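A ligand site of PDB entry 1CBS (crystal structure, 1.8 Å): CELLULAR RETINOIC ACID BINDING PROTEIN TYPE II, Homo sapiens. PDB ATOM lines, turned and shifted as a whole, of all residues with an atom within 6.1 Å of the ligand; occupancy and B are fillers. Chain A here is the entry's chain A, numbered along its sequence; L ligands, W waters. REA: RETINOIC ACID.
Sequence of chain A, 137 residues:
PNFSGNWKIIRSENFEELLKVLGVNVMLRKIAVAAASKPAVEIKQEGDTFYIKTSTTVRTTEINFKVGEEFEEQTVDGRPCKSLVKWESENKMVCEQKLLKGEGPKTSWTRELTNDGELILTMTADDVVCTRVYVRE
Merely in contact with the ligand: Leu 121, Ala 32, Thr 54, Val 58, Val 76, Leu 19, Thr 56, Pro 39, Phe 15, Asp 77, Ala 36, Ile 31 and Arg 59. The nearest printed residue that does not touch the ligand is Leu 28 (4.1 Å).
Water W1 lies within hydrogen-bond range of O2 of the ligand (2.7 Å), OG1 of Thr 54 (3.0 Å) and NH2 of Arg 111 (3.0 Å).
O of Arg 59 lies within hydrogen-bond range of OG1 of Thr 56, 2.8 Å away. The backbone NH of Leu 121 lies within hydrogen-bond range of the backbone carbonyl oxygen of Arg 132 (2.8 Å). The guanidinium group (NH2) of Arg 132 lies within hydrogen-bond range of the backbone carbonyl oxygen (O) of Ala 36. The backbone NH of Val 24 is in hydrogen-bond range of the backbone carbonyl oxygen of Leu 19, at 3.1 Å. The backbone NH (N) of Val 58 sits close to the side-chain hydroxyl (OG1) of Thr 56, at 3.4 Å.
The guanidinium group of Arg 132 is in salt-bridge range of an oxygen (O1) of the ligand, at 2.7 Å. An oxygen (O1) of the ligand is in hydrogen-bond range of the side-chain hydroxyl (OH) of Tyr 134 (2.6 Å).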
ATOM      1  N   ILE A   9     -21.552 -33.646 -36.107  1.00  0.00           N
ATOM      2  CA  ILE A   9     -21.067 -32.297 -36.386  1.00  0.00           C
ATOM      3  C   ILE A   9     -19.989 -32.240 -37.475  1.00  0.00           C
ATOM      4  O   ILE A   9     -19.191 -33.174 -37.608  1.00  0.00           O
ATOM      5  CB  ILE A   9     -20.568 -31.645 -35.063  1.00  0.00           C
ATOM      6  CG1 ILE A   9     -20.441 -30.128 -35.222  1.00  0.00           C
ATOM      7  CG2 ILE A   9     -19.244 -32.246 -34.643  1.00  0.00           C
ATOM      8  CD1 ILE A   9     -20.090 -29.462 -33.914  1.00  0.00           C
ATOM      9  N   PHE A  15     -17.285 -21.541 -30.020  1.00  0.00           N
ATOM     10  CA  PHE A  15     -17.816 -22.193 -28.815  1.00  0.00           C
ATOM     11  C   PHE A  15     -17.148 -21.733 -27.525  1.00  0.00           C
ATOM     12  O   PHE A  15     -17.823 -21.423 -26.551  1.00  0.00           O
ATOM     13  CB  PHE A  15     -17.718 -23.726 -28.914  1.00  0.00           C
ATOM     14  CG  PHE A  15     -18.452 -24.448 -27.806  1.00  0.00           C
ATOM     15  CD1 PHE A  15     -19.815 -24.271 -27.631  1.00  0.00           C
ATOM     16  CD2 PHE A  15     -17.767 -25.306 -26.961  1.00  0.00           C
ATOM     17  CE1 PHE A  15     -20.500 -24.962 -26.630  1.00  0.00           C
ATOM     18  CE2 PHE A  15     -18.438 -25.999 -25.959  1.00  0.00           C
ATOM     19  CZ  PHE A  15     -19.809 -25.827 -25.788  1.00  0.00           C
ATOM     20  N   LEU A  19     -18.645 -19.566 -24.135  1.00  0.00           N
ATOM     21  CA  LEU A  19     -18.478 -19.983 -22.741  1.00  0.00           C
ATOM     22  C   LEU A  19     -17.812 -18.892 -21.894  1.00  0.00           C
ATOM     23  O   LEU A  19     -18.130 -18.739 -20.710  1.00  0.00           O
ATOM     24  CB  LEU A  19     -17.676 -21.288 -22.654  1.00  0.00           C
ATOM     25  CG  LEU A  19     -18.306 -22.557 -23.249  1.00  0.00           C
ATOM     26  CD1 LEU A  19     -17.405 -23.756 -22.958  1.00  0.00           C
ATOM     27  CD2 LEU A  19     -19.718 -22.787 -22.690  1.00  0.00           C
ATOM     28  N   VAL A  24     -17.682 -19.034 -17.689  1.00  0.00           N
ATOM     29  CA  VAL A  24     -17.073 -20.305 -17.350  1.00  0.00           C
ATOM     30  C   VAL A  24     -15.551 -20.128 -17.283  1.00  0.00           C
ATOM     31  O   VAL A  24     -14.929 -19.598 -18.211  1.00  0.00           O
ATOM     32  CB  VAL A  24     -17.445 -21.392 -18.391  1.00  0.00           C
ATOM     33  CG1 VAL A  24     -16.802 -22.709 -18.018  1.00  0.00           C
ATOM     34  CG2 VAL A  24     -18.980 -21.520 -18.488  1.00  0.00           C
ATOM     35  N   LEU A  28     -12.506 -25.236 -16.747  1.00  0.00           N
ATOM     36  CA  LEU A  28     -13.778 -25.868 -17.072  1.00  0.00           C
ATOM     37  C   LEU A  28     -14.017 -25.719 -18.571  1.00  0.00           C
ATOM     38  O   LEU A  28     -14.566 -26.619 -19.199  1.00  0.00           O
ATOM     39  CB  LEU A  28     -14.938 -25.268 -16.260  1.00  0.00           C
ATOM     40  CG  LEU A  28     -15.030 -25.774 -14.812  1.00  0.00           C
ATOM     41  CD1 LEU A  28     -16.073 -25.009 -14.011  1.00  0.00           C
ATOM     42  CD2 LEU A  28     -15.317 -27.279 -14.797  1.00  0.00           C
ATOM     43  N   ILE A  31     -12.154 -28.412 -20.561  1.00  0.00           N
ATOM     44  CA  ILE A  31     -12.878 -29.684 -20.491  1.00  0.00           C
ATOM     45  C   ILE A  31     -14.093 -29.667 -21.435  1.00  0.00           C
ATOM     46  O   ILE A  31     -14.269 -30.599 -22.219  1.00  0.00           O
ATOM     47  CB  ILE A  31     -13.381 -29.947 -19.041  1.00  0.00           C
ATOM     48  CG1 ILE A  31     -12.186 -30.107 -18.091  1.00  0.00           C
ATOM     49  CG2 ILE A  31     -14.303 -31.163 -18.990  1.00  0.00           C
ATOM     50  CD1 ILE A  31     -12.555 -30.261 -16.601  1.00  0.00           C
ATOM     51  N   ALA A  32     -14.891 -28.610 -21.363  1.00  0.00           N
ATOM     52  CA  ALA A  32     -16.100 -28.480 -22.175  1.00  0.00           C
ATOM     53  C   ALA A  32     -15.829 -28.476 -23.677  1.00  0.00           C
ATOM     54  O   ALA A  32     -16.483 -29.209 -24.415  1.00  0.00           O
ATOM     55  CB  ALA A  32     -16.853 -27.218 -21.763  1.00  0.00           C
ATOM     56  N   VAL A  33     -14.871 -27.684 -24.125  1.00  0.00           N
ATOM     57  CA  VAL A  33     -14.531 -27.598 -25.544  1.00  0.00           C
ATOM     58  C   VAL A  33     -14.095 -28.935 -26.164  1.00  0.00           C
ATOM     59  O   VAL A  33     -14.493 -29.260 -27.273  1.00  0.00           O
ATOM     60  CB  VAL A  33     -13.424 -26.509 -25.802  1.00  0.00           C
ATOM     61  CG1 VAL A  33     -12.933 -26.582 -27.235  1.00  0.00           C
ATOM     62  CG2 VAL A  33     -14.000 -25.124 -25.519  1.00  0.00           C
ATOM     63  N   ALA A  35     -14.854 -32.037 -25.063  1.00  0.00           N
ATOM     64  CA  ALA A  35     -15.991 -32.936 -25.097  1.00  0.00           C
ATOM     65  C   ALA A  35     -17.031 -32.539 -26.148  1.00  0.00           C
ATOM     66  O   ALA A  35     -17.614 -33.394 -26.811  1.00  0.00           O
ATOM     67  CB  ALA A  35     -16.631 -33.039 -23.717  1.00  0.00           C
ATOM     68  N   ALA A  36     -17.225 -31.234 -26.328  1.00  0.00           N
ATOM     69  CA  ALA A  36     -18.217 -30.740 -27.277  1.00  0.00           C
ATOM     70  C   ALA A  36     -17.824 -30.876 -28.746  1.00  0.00           C
ATOM     71  O   ALA A  36     -18.645 -30.611 -29.630  1.00  0.00           O
ATOM     72  CB  ALA A  36     -18.564 -29.294 -26.972  1.00  0.00           C
ATOM     73  N   PRO A  39     -20.055 -34.474 -30.392  1.00  0.00           N
ATOM     74  CA  PRO A  39     -21.339 -34.834 -29.779  1.00  0.00           C
ATOM     75  C   PRO A  39     -22.147 -35.848 -30.583  1.00  0.00           C
ATOM     76  O   PRO A  39     -21.894 -36.062 -31.772  1.00  0.00           O
ATOM     77  CB  PRO A  39     -22.074 -33.499 -29.746  1.00  0.00           C
ATOM     78  CG  PRO A  39     -21.628 -32.853 -30.982  1.00  0.00           C
ATOM     79  CD  PRO A  39     -20.147 -33.186 -31.101  1.00  0.00           C
ATOM     80  N   VAL A  41     -25.953 -36.399 -31.526  1.00  0.00           N
ATOM     81  CA  VAL A  41     -27.235 -35.684 -31.447  1.00  0.00           C
ATOM     82  C   VAL A  41     -28.353 -36.513 -32.073  1.00  0.00           C
ATOM     83  O   VAL A  41     -28.231 -36.972 -33.212  1.00  0.00           O
ATOM     84  CB  VAL A  41     -27.170 -34.323 -32.201  1.00  0.00           C
ATOM     85  CG1 VAL A  41     -28.515 -33.594 -32.123  1.00  0.00           C
ATOM     86  CG2 VAL A  41     -26.070 -33.445 -31.617  1.00  0.00           C
ATOM     87  N   THR A  54     -28.691 -34.435 -26.744  1.00  0.00           N
ATOM     88  CA  THR A  54     -27.341 -34.094 -27.123  1.00  0.00           C
ATOM     89  C   THR A  54     -26.425 -34.724 -26.087  1.00  0.00           C
ATOM     90  O   THR A  54     -26.481 -34.385 -24.910  1.00  0.00           O
ATOM     91  CB  THR A  54     -27.146 -32.587 -27.166  1.00  0.00           C
ATOM     92  OG1 THR A  54     -28.142 -32.019 -28.013  1.00  0.00           O
ATOM     93  CG2 THR A  54     -25.769 -32.253 -27.731  1.00  0.00           C
ATOM     94  N   SER A  55     -25.568 -35.614 -26.550  1.00  0.00           N
ATOM     95  CA  SER A  55     -24.705 -36.351 -25.662  1.00  0.00           C
ATOM     96  C   SER A  55     -23.199 -36.186 -25.878  1.00  0.00           C
ATOM     97  O   SER A  55     -22.727 -36.128 -27.009  1.00  0.00           O
ATOM     98  CB  SER A  55     -25.094 -37.824 -25.752  1.00  0.00           C
ATOM     99  OG  SER A  55     -24.219 -38.654 -25.002  1.00  0.00           O
ATOM    100  N   THR A  56     -22.475 -36.039 -24.766  1.00  0.00           N
ATOM    101  CA  THR A  56     -21.009 -35.942 -24.765  1.00  0.00           C
ATOM    102  C   THR A  56     -20.533 -36.760 -23.542  1.00  0.00           C
ATOM    103  O   THR A  56     -21.324 -37.155 -22.695  1.00  0.00           O
ATOM    104  CB  THR A  56     -20.482 -34.477 -24.631  1.00  0.00           C
ATOM    105  OG1 THR A  56     -20.791 -33.977 -23.321  1.00  0.00           O
ATOM    106  CG2 THR A  56     -21.116 -33.559 -25.661  1.00  0.00           C
ATOM    107  N   VAL A  58     -19.032 -35.786 -20.982  1.00  0.00           N
ATOM    108  CA  VAL A  58     -19.162 -35.007 -19.727  1.00  0.00           C
ATOM    109  C   VAL A  58     -20.540 -34.434 -19.395  1.00  0.00           C
ATOM    110  O   VAL A  58     -20.769 -33.977 -18.276  1.00  0.00           O
ATOM    111  CB  VAL A  58     -18.136 -33.824 -19.696  1.00  0.00           C
ATOM    112  CG1 VAL A  58     -16.690 -34.331 -19.970  1.00  0.00           C
ATOM    113  CG2 VAL A  58     -18.504 -32.738 -20.722  1.00  0.00           C
ATOM    114  N   ARG A  59     -21.479 -34.490 -20.342  1.00  0.00           N
ATOM    115  CA  ARG A  59     -22.799 -33.923 -20.116  1.00  0.00           C
ATOM    116  C   ARG A  59     -23.746 -34.337 -21.222  1.00  0.00           C
ATOM    117  O   ARG A  59     -23.405 -34.266 -22.391  1.00  0.00           O
ATOM    118  CB  ARG A  59     -22.681 -32.389 -20.128  1.00  0.00           C
ATOM    119  CG  ARG A  59     -23.991 -31.601 -20.014  1.00  0.00           C
ATOM    120  CD  ARG A  59     -23.687 -30.138 -19.673  1.00  0.00           C
ATOM    121  NE  ARG A  59     -24.808 -29.225 -19.859  1.00  0.00           N
ATOM    122  CZ  ARG A  59     -25.744 -28.984 -18.955  1.00  0.00           C
ATOM    123  NH1 ARG A  59     -25.709 -29.584 -17.764  1.00  0.00           N
ATOM    124  NH2 ARG A  59     -26.754 -28.160 -19.248  1.00  0.00           N
ATOM    125  N   VAL A  76     -26.540 -23.267 -21.745  1.00  0.00           N
ATOM    126  CA  VAL A  76     -25.359 -24.086 -22.089  1.00  0.00           C
ATOM    127  C   VAL A  76     -24.430 -24.325 -20.894  1.00  0.00           C
ATOM    128  O   VAL A  76     -23.891 -25.426 -20.744  1.00  0.00           O
ATOM    129  CB  VAL A  76     -24.528 -23.465 -23.251  1.00  0.00           C
ATOM    130  CG1 VAL A  76     -23.664 -24.516 -23.903  1.00  0.00           C
ATOM    131  CG2 VAL A  76     -25.426 -22.860 -24.291  1.00  0.00           C
ATOM    132  N   ASP A  77     -24.278 -23.321 -20.038  1.00  0.00           N
ATOM    133  CA  ASP A  77     -23.432 -23.443 -18.848  1.00  0.00           C
ATOM    134  C   ASP A  77     -24.121 -24.108 -17.655  1.00  0.00           C
ATOM    135  O   ASP A  77     -23.578 -24.135 -16.550  1.00  0.00           O
ATOM    136  CB  ASP A  77     -22.801 -22.084 -18.474  1.00  0.00           C
ATOM    137  CG  ASP A  77     -23.824 -21.030 -18.083  1.00  0.00           C
ATOM    138  OD1 ASP A  77     -24.847 -20.845 -18.799  1.00  0.00           O
ATOM    139  OD2 ASP A  77     -23.593 -20.355 -17.063  1.00  0.00           O
ATOM    140  N   GLY A  78     -25.345 -24.597 -17.882  1.00  0.00           N
ATOM    141  CA  GLY A  78     -26.101 -25.314 -16.850  1.00  0.00           C
ATOM    142  C   GLY A  78     -27.085 -24.624 -15.918  1.00  0.00           C
ATOM    143  O   GLY A  78     -27.471 -25.210 -14.902  1.00  0.00           O
ATOM    144  N   ARG A 111     -32.397 -23.285 -34.497  1.00  0.00           N
ATOM    145  CA  ARG A 111     -32.074 -24.518 -35.236  1.00  0.00           C
ATOM    146  C   ARG A 111     -32.747 -24.371 -36.576  1.00  0.00           C
ATOM    147  O   ARG A 111     -33.904 -23.973 -36.654  1.00  0.00           O
ATOM    148  CB  ARG A 111     -32.572 -25.790 -34.544  1.00  0.00           C
ATOM    149  CG  ARG A 111     -31.665 -26.217 -33.400  1.00  0.00           C
ATOM    150  CD  ARG A 111     -32.086 -27.556 -32.805  1.00  0.00           C
ATOM    151  NE  ARG A 111     -31.059 -28.071 -31.890  1.00  0.00           N
ATOM    152  CZ  ARG A 111     -30.969 -27.753 -30.604  1.00  0.00           C
ATOM    153  NH1 ARG A 111     -31.847 -26.920 -30.073  1.00  0.00           N
ATOM    154  NH2 ARG A 111     -30.019 -28.279 -29.835  1.00  0.00           N
ATOM    155  N   LEU A 121     -27.131 -24.963 -36.014  1.00  0.00           N
ATOM    156  CA  LEU A 121     -27.512 -24.594 -34.649  1.00  0.00           C
ATOM    157  C   LEU A 121     -26.742 -23.318 -34.285  1.00  0.00           C
ATOM    158  O   LEU A 121     -25.547 -23.214 -34.562  1.00  0.00           O
ATOM    159  CB  LEU A 121     -27.114 -25.684 -33.646  1.00  0.00           C
ATOM    160  CG  LEU A 121     -27.070 -25.270 -32.150  1.00  0.00           C
ATOM    161  CD1 LEU A 121     -28.487 -25.063 -31.577  1.00  0.00           C
ATOM    162  CD2 LEU A 121     -26.316 -26.318 -31.328  1.00  0.00           C
ATOM    163  N   MET A 123     -26.070 -20.563 -31.054  1.00  0.00           N
ATOM    164  CA  MET A 123     -26.292 -20.311 -29.633  1.00  0.00           C
ATOM    165  C   MET A 123     -25.801 -18.895 -29.392  1.00  0.00           C
ATOM    166  O   MET A 123     -24.726 -18.532 -29.889  1.00  0.00           O
ATOM    167  CB  MET A 123     -25.546 -21.340 -28.775  1.00  0.00           C
ATOM    168  CG  MET A 123     -26.123 -22.740 -28.896  1.00  0.00           C
ATOM    169  SD  MET A 123     -25.318 -23.967 -27.846  1.00  0.00           S
ATOM    170  CE  MET A 123     -23.835 -24.323 -28.800  1.00  0.00           C
ATOM    171  N   ARG A 132     -22.788 -23.947 -35.179  1.00  0.00           N
ATOM    172  CA  ARG A 132     -22.421 -25.358 -35.318  1.00  0.00           C
ATOM    173  C   ARG A 132     -23.252 -25.938 -36.461  1.00  0.00           C
ATOM    174  O   ARG A 132     -24.453 -25.669 -36.551  1.00  0.00           O
ATOM    175  CB  ARG A 132     -22.689 -26.134 -34.020  1.00  0.00           C
ATOM    176  CG  ARG A 132     -22.381 -25.345 -32.769  1.00  0.00           C
ATOM    177  CD  ARG A 132     -21.236 -25.909 -31.993  1.00  0.00           C
ATOM    178  NE  ARG A 132     -21.559 -27.146 -31.295  1.00  0.00           N
ATOM    179  CZ  ARG A 132     -20.658 -27.925 -30.703  1.00  0.00           C
ATOM    180  NH1 ARG A 132     -19.372 -27.581 -30.705  1.00  0.00           N
ATOM    181  NH2 ARG A 132     -20.999 -29.093 -30.194  1.00  0.00           N
ATOM    182  N   TYR A 134     -24.316 -29.511 -38.731  1.00  0.00           N
ATOM    183  CA  TYR A 134     -24.347 -30.959 -38.667  1.00  0.00           C
ATOM    184  C   TYR A 134     -24.923 -31.531 -39.946  1.00  0.00           C
ATOM    185  O   TYR A 134     -25.618 -30.842 -40.691  1.00  0.00           O
ATOM    186  CB  TYR A 134     -25.257 -31.436 -37.527  1.00  0.00           C
ATOM    187  CG  TYR A 134     -24.995 -30.822 -36.173  1.00  0.00           C
ATOM    188  CD1 TYR A 134     -25.387 -29.514 -35.913  1.00  0.00           C
ATOM    189  CD2 TYR A 134     -24.393 -31.555 -35.153  1.00  0.00           C
ATOM    190  CE1 TYR A 134     -25.186 -28.949 -34.691  1.00  0.00           C
ATOM    191  CE2 TYR A 134     -24.185 -30.979 -33.910  1.00  0.00           C
ATOM    192  CZ  TYR A 134     -24.594 -29.674 -33.705  1.00  0.00           C
ATOM    193  OH  TYR A 134     -24.402 -29.037 -32.520  1.00  0.00           O
HETATM  194  C1  REA L   1     -19.146 -28.753 -18.055  1.00  0.00           C
HETATM  195  C2  REA L   1     -19.255 -28.025 -16.696  1.00  0.00           C
HETATM  196  C3  REA L   1     -18.838 -26.596 -16.694  1.00  0.00           C
HETATM  197  C4  REA L   1     -19.596 -25.778 -17.681  1.00  0.00           C
HETATM  198  C5  REA L   1     -19.782 -26.466 -19.037  1.00  0.00           C
HETATM  199  C6  REA L   1     -19.669 -27.819 -19.192  1.00  0.00           C
HETATM  200  C7  REA L   1     -19.856 -28.531 -20.479  1.00  0.00           C
HETATM  201  C8  REA L   1     -20.677 -28.229 -21.485  1.00  0.00           C
HETATM  202  C9  REA L   1     -20.842 -28.962 -22.722  1.00  0.00           C
HETATM  203  C10 REA L   1     -21.696 -28.488 -23.636  1.00  0.00           C
HETATM  204  C11 REA L   1     -21.960 -29.132 -24.912  1.00  0.00           C
HETATM  205  C12 REA L   1     -22.820 -28.553 -25.752  1.00  0.00           C
HETATM  206  C13 REA L   1     -23.167 -29.127 -27.030  1.00  0.00           C
HETATM  207  C14 REA L   1     -24.039 -28.460 -27.834  1.00  0.00           C
HETATM  208  C15 REA L   1     -24.546 -28.865 -29.156  1.00  0.00           C
HETATM  209  C16 REA L   1     -19.999 -30.031 -17.988  1.00  0.00           C
HETATM  210  C17 REA L   1     -17.667 -29.136 -18.334  1.00  0.00           C
HETATM  211  C18 REA L   1     -20.251 -25.453 -20.083  1.00  0.00           C
HETATM  212  C19 REA L   1     -20.009 -30.231 -22.976  1.00  0.00           C
HETATM  213  C20 REA L   1     -22.556 -30.474 -27.429  1.00  0.00           C
HETATM  214  O1  REA L   1     -23.724 -29.202 -30.037  1.00  0.00           O
HETATM  215  O2  REA L   1     -25.776 -28.870 -29.372  1.00  0.00           O
HETATM  216  O   HOH W   1     -27.826 -30.264 -30.440  1.00  0.00           O
HETATM  217  O   HOH W   2     -27.411 -28.336 -26.926  1.00  0.00           O
